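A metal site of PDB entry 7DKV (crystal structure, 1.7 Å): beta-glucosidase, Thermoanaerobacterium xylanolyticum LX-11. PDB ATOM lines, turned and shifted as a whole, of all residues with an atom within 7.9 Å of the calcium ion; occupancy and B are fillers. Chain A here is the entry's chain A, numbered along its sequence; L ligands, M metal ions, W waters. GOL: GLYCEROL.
The backbone NH of Asn 563 lies close to the side-chain carboxylate of Asp 560, at 3.3 Å.
The side-chain amide nitrogen (ND2) of Asn 626 sits at hydrogen-bond distance from the backbone carbonyl oxygen (O) of Asp 564 (2.8 Å).
The side-chain carboxylate (OD2) of Asp 564 sits close to the side-chain carboxylate (OE2) of Glu 630, at 2.7 Å.
The side-chain carboxylate (OD2) of Asp 564 lies within hydrogen-bond range of the side-chain hydroxyl (OG1) of Thr 585, 3.0 Å away.
N of Asp 568 lies within hydrogen-bond range of O of Met 559.
The backbone NH (N) of Lys 561 sits close to the side-chain carboxylate (OD1) of Asp 568 (2.9 Å).
N of Gly 565 is in hydrogen-bond range of OD2 of Asp 560, at 2.8 Å.
The calcium ion is bound by the side-chain carboxylate (OD1) of Asp 568 (2.3 Å), the side-chain carboxylate (OD1) of Asp 564 (2.3 Å), the backbone carbonyl oxygen (O) of Ile 566 (2.4 Å), water W1 (2.4 Å), the side-chain carboxylate (OD1) of Asp 560 (2.5 Å), the side-chain carboxylate (OD1) of Asp 562 (2.5 Å) and an oxygen (O3) of the ligand (2.8 Å).
The calcium ion has seven donor atoms within binding distance.
Water W1 bridges OG1 of Thr 585 and O of Pro 567.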
ATOM      1  N   LYS A 557      -8.736  10.303   7.646  1.00  0.00           N
ATOM      2  CA  LYS A 557      -8.139   9.649   6.467  1.00  0.00           C
ATOM      3  C   LYS A 557      -9.229   9.261   5.448  1.00  0.00           C
ATOM      4  O   LYS A 557      -9.007   9.364   4.240  1.00  0.00           O
ATOM      5  CB  LYS A 557      -7.332   8.424   6.895  1.00  0.00           C
ATOM      6  CG  LYS A 557      -6.562   7.678   5.797  1.00  0.00           C
ATOM      7  CD  LYS A 557      -5.607   8.586   5.038  1.00  0.00           C
ATOM      8  CE  LYS A 557      -4.485   7.810   4.384  1.00  0.00           C
ATOM      9  NZ  LYS A 557      -4.966   6.718   3.520  1.00  0.00           N
ATOM     10  N   MET A 559     -11.749  10.906   4.580  1.00  0.00           N
ATOM     11  CA  MET A 559     -12.116  12.092   3.792  1.00  0.00           C
ATOM     12  C   MET A 559     -11.145  12.413   2.658  1.00  0.00           C
ATOM     13  O   MET A 559     -11.320  13.396   1.946  1.00  0.00           O
ATOM     14  CB  MET A 559     -12.298  13.289   4.725  1.00  0.00           C
ATOM     15  CG  MET A 559     -13.490  13.147   5.643  1.00  0.00           C
ATOM     16  SD  MET A 559     -13.459  14.359   6.970  1.00  0.00           S
ATOM     17  CE  MET A 559     -14.984  13.905   7.784  1.00  0.00           C
ATOM     18  N   ASP A 560     -10.125  11.586   2.470  1.00  0.00           N
ATOM     19  CA  ASP A 560      -9.265  11.649   1.287  1.00  0.00           C
ATOM     20  C   ASP A 560     -10.038  11.048   0.115  1.00  0.00           C
ATOM     21  O   ASP A 560     -10.205   9.844   0.066  1.00  0.00           O
ATOM     22  CB  ASP A 560      -7.973  10.869   1.548  1.00  0.00           C
ATOM     23  CG  ASP A 560      -7.022  10.858   0.368  1.00  0.00           C
ATOM     24  OD1 ASP A 560      -7.185  11.674  -0.551  1.00  0.00           O
ATOM     25  OD2 ASP A 560      -6.100  10.030   0.385  1.00  0.00           O
ATOM     26  N   LYS A 561     -10.512  11.897  -0.781  1.00  0.00           N
ATOM     27  CA  LYS A 561     -11.341  11.474  -1.927  1.00  0.00           C
ATOM     28  C   LYS A 561     -10.550  10.871  -3.098  1.00  0.00           C
ATOM     29  O   LYS A 561     -11.112  10.090  -3.878  1.00  0.00           O
ATOM     30  CB  LYS A 561     -12.140  12.658  -2.468  1.00  0.00           C
ATOM     31  CG  LYS A 561     -13.234  13.174  -1.562  1.00  0.00           C
ATOM     32  CD  LYS A 561     -13.791  14.480  -2.113  1.00  0.00           C
ATOM     33  CE  LYS A 561     -15.064  14.911  -1.414  1.00  0.00           C
ATOM     34  NZ  LYS A 561     -15.563  16.199  -1.967  1.00  0.00           N
ATOM     35  N   ASP A 562      -9.280  11.225  -3.249  1.00  0.00           N
ATOM     36  CA  ASP A 562      -8.525  10.922  -4.474  1.00  0.00           C
ATOM     37  C   ASP A 562      -7.227  10.149  -4.223  1.00  0.00           C
ATOM     38  O   ASP A 562      -6.350  10.102  -5.096  1.00  0.00           O
ATOM     39  CB  ASP A 562      -8.258  12.214  -5.238  1.00  0.00           C
ATOM     40  CG  ASP A 562      -7.319  13.139  -4.494  1.00  0.00           C
ATOM     41  OD1 ASP A 562      -7.142  12.966  -3.260  1.00  0.00           O
ATOM     42  OD2 ASP A 562      -6.757  14.049  -5.126  1.00  0.00           O
ATOM     43  N   ASN A 563      -7.101   9.558  -3.041  1.00  0.00           N
ATOM     44  CA  ASN A 563      -5.941   8.777  -2.640  1.00  0.00           C
ATOM     45  C   ASN A 563      -4.570   9.470  -2.799  1.00  0.00           C
ATOM     46  O   ASN A 563      -3.574   8.814  -3.093  1.00  0.00           O
ATOM     47  CB  ASN A 563      -5.955   7.395  -3.346  1.00  0.00           C
ATOM     48  CG  ASN A 563      -5.189   6.320  -2.577  1.00  0.00           C
ATOM     49  OD1 ASN A 563      -5.071   6.363  -1.348  1.00  0.00           O
ATOM     50  ND2 ASN A 563      -4.663   5.346  -3.304  1.00  0.00           N
ATOM     51  N   ASP A 564      -4.503  10.785  -2.577  1.00  0.00           N
ATOM     52  CA  ASP A 564      -3.196  11.479  -2.443  1.00  0.00           C
ATOM     53  C   ASP A 564      -2.673  11.448  -0.984  1.00  0.00           C
ATOM     54  O   ASP A 564      -1.614  12.024  -0.697  1.00  0.00           O
ATOM     55  CB  ASP A 564      -3.262  12.904  -3.007  1.00  0.00           C
ATOM     56  CG  ASP A 564      -3.894  13.918  -2.038  1.00  0.00           C
ATOM     57  OD1 ASP A 564      -4.664  13.516  -1.156  1.00  0.00           O
ATOM     58  OD2 ASP A 564      -3.622  15.118  -2.176  1.00  0.00           O
ATOM     59  N   GLY A 565      -3.416  10.791  -0.077  1.00  0.00           N
ATOM     60  CA  GLY A 565      -3.029  10.618   1.318  1.00  0.00           C
ATOM     61  C   GLY A 565      -3.442  11.768   2.246  1.00  0.00           C
ATOM     62  O   GLY A 565      -3.080  11.760   3.414  1.00  0.00           O
ATOM     63  N   ILE A 566      -4.203  12.734   1.716  1.00  0.00           N
ATOM     64  CA  ILE A 566      -4.561  13.958   2.440  1.00  0.00           C
ATOM     65  C   ILE A 566      -6.078  14.139   2.369  1.00  0.00           C
ATOM     66  O   ILE A 566      -6.673  13.991   1.295  1.00  0.00           O
ATOM     67  CB  ILE A 566      -3.844  15.180   1.817  1.00  0.00           C
ATOM     68  CG1 ILE A 566      -2.328  14.936   1.706  1.00  0.00           C
ATOM     69  CG2 ILE A 566      -4.112  16.436   2.653  1.00  0.00           C
ATOM     70  CD1 ILE A 566      -1.599  15.976   0.905  1.00  0.00           C
ATOM     71  N   PRO A 567      -6.741  14.444   3.511  1.00  0.00           N
ATOM     72  CA  PRO A 567      -8.171  14.765   3.398  1.00  0.00           C
ATOM     73  C   PRO A 567      -8.468  15.910   2.434  1.00  0.00           C
ATOM     74  O   PRO A 567      -7.655  16.830   2.280  1.00  0.00           O
ATOM     75  CB  PRO A 567      -8.580  15.128   4.836  1.00  0.00           C
ATOM     76  CG  PRO A 567      -7.304  15.461   5.528  1.00  0.00           C
ATOM     77  CD  PRO A 567      -6.237  14.640   4.879  1.00  0.00           C
ATOM     78  N   ASP A 568      -9.590  15.806   1.717  1.00  0.00           N
ATOM     79  CA  ASP A 568      -9.998  16.821   0.749  1.00  0.00           C
ATOM     80  C   ASP A 568     -10.950  17.836   1.375  1.00  0.00           C
ATOM     81  O   ASP A 568     -12.032  17.461   1.840  1.00  0.00           O
ATOM     82  CB  ASP A 568     -10.724  16.178  -0.438  1.00  0.00           C
ATOM     83  CG  ASP A 568      -9.785  15.410  -1.347  1.00  0.00           C
ATOM     84  OD1 ASP A 568      -9.151  14.422  -0.891  1.00  0.00           O
ATOM     85  OD2 ASP A 568      -9.675  15.805  -2.520  1.00  0.00           O
ATOM     86  N   ASN A 569     -10.597  19.120   1.333  1.00  0.00           N
ATOM     87  CA  ASN A 569     -11.566  20.182   1.628  1.00  0.00           C
ATOM     88  C   ASN A 569     -12.624  20.166   0.502  1.00  0.00           C
ATOM     89  O   ASN A 569     -12.306  19.922  -0.664  1.00  0.00           O
ATOM     90  CB  ASN A 569     -10.877  21.545   1.720  1.00  0.00           C
ATOM     91  CG  ASN A 569      -9.928  21.642   2.916  1.00  0.00           C
ATOM     92  OD1 ASN A 569      -8.719  21.471   2.772  1.00  0.00           O
ATOM     93  ND2 ASN A 569     -10.468  21.925   4.088  1.00  0.00           N
ATOM     94  N   GLY A 584      -9.933  20.737  -2.156  1.00  0.00           N
ATOM     95  CA  GLY A 584      -8.837  19.838  -2.444  1.00  0.00           C
ATOM     96  C   GLY A 584      -7.864  19.789  -1.277  1.00  0.00           C
ATOM     97  O   GLY A 584      -8.286  19.676  -0.117  1.00  0.00           O
ATOM     98  N   THR A 585      -6.578  19.882  -1.586  1.00  0.00           N
ATOM     99  CA  THR A 585      -5.554  19.895  -0.547  1.00  0.00           C
ATOM    100  C   THR A 585      -5.283  21.345  -0.220  1.00  0.00           C
ATOM    101  O   THR A 585      -4.946  22.118  -1.104  1.00  0.00           O
ATOM    102  CB  THR A 585      -4.267  19.182  -1.016  1.00  0.00           C
ATOM    103  OG1 THR A 585      -4.535  17.780  -1.124  1.00  0.00           O
ATOM    104  CG2 THR A 585      -3.113  19.397  -0.026  1.00  0.00           C
ATOM    105  N   ASN A 626       3.257  14.394  -1.225  1.00  0.00           N
ATOM    106  CA  ASN A 626       2.205  14.968  -2.060  1.00  0.00           C
ATOM    107  C   ASN A 626       1.839  16.409  -1.706  1.00  0.00           C
ATOM    108  O   ASN A 626       1.498  17.177  -2.592  1.00  0.00           O
ATOM    109  CB  ASN A 626       0.969  14.073  -2.047  1.00  0.00           C
ATOM    110  CG  ASN A 626       1.172  12.810  -2.864  1.00  0.00           C
ATOM    111  OD1 ASN A 626       1.963  12.794  -3.798  1.00  0.00           O
ATOM    112  ND2 ASN A 626       0.441  11.761  -2.523  1.00  0.00           N
ATOM    113  N   GLU A 630       2.033  19.271  -4.592  1.00  0.00           N
ATOM    114  CA  GLU A 630       0.814  19.968  -4.934  1.00  0.00           C
ATOM    115  C   GLU A 630       0.848  21.467  -4.668  1.00  0.00           C
ATOM    116  O   GLU A 630       0.265  22.234  -5.434  1.00  0.00           O
ATOM    117  CB  GLU A 630      -0.364  19.354  -4.169  1.00  0.00           C
ATOM    118  CG  GLU A 630      -0.773  17.975  -4.672  1.00  0.00           C
ATOM    119  CD  GLU A 630      -1.612  17.203  -3.681  1.00  0.00           C
ATOM    120  OE1 GLU A 630      -2.202  17.839  -2.771  1.00  0.00           O
ATOM    121  OE2 GLU A 630      -1.693  15.956  -3.803  1.00  0.00           O
ATOM    122  N   THR A 641      -5.433  23.484  -3.764  1.00  0.00           N
ATOM    123  CA  THR A 641      -5.250  22.932  -5.107  1.00  0.00           C
ATOM    124  C   THR A 641      -6.406  23.174  -6.083  1.00  0.00           C
ATOM    125  O   THR A 641      -6.212  23.029  -7.289  1.00  0.00           O
ATOM    126  CB  THR A 641      -4.994  21.423  -5.043  1.00  0.00           C
ATOM    127  OG1 THR A 641      -6.091  20.787  -4.377  1.00  0.00           O
ATOM    128  CG2 THR A 641      -3.684  21.131  -4.339  1.00  0.00           C
ATOM    129  N   GLU A 642      -7.607  23.516  -5.587  1.00  0.00           N
ATOM    130  CA  GLU A 642      -8.811  23.571  -6.450  1.00  0.00           C
ATOM    131  C   GLU A 642      -9.693  24.837  -6.417  1.00  0.00           C
ATOM    132  O   GLU A 642     -10.609  24.956  -7.222  1.00  0.00           O
ATOM    133  CB  GLU A 642      -9.678  22.338  -6.184  1.00  0.00           C
ATOM    134  CG  GLU A 642      -9.012  21.030  -6.586  1.00  0.00           C
ATOM    135  CD  GLU A 642      -9.895  19.816  -6.353  1.00  0.00           C
ATOM    136  OE1 GLU A 642     -11.133  19.925  -6.502  1.00  0.00           O
ATOM    137  OE2 GLU A 642      -9.365  18.739  -6.010  1.00  0.00           O
HETATM  138  C1  GOL L   1      -4.709  17.329  -4.995  1.00  0.00           C
HETATM  139  O1  GOL L   1      -4.114  17.576  -6.269  1.00  0.00           O
HETATM  140  C2  GOL L   1      -6.227  17.291  -5.174  1.00  0.00           C
HETATM  141  O2  GOL L   1      -6.671  18.567  -5.638  1.00  0.00           O
HETATM  142  C3  GOL L   1      -6.967  16.957  -3.879  1.00  0.00           C
HETATM  143  O3  GOL L   1      -6.436  15.827  -3.181  1.00  0.00           O
HETATM  144 CA    CA M   1      -6.902  14.058  -1.065  1.00  0.00          CA
HETATM  145  O   HOH W   1      -6.611  16.404  -0.459  1.00  0.00           O
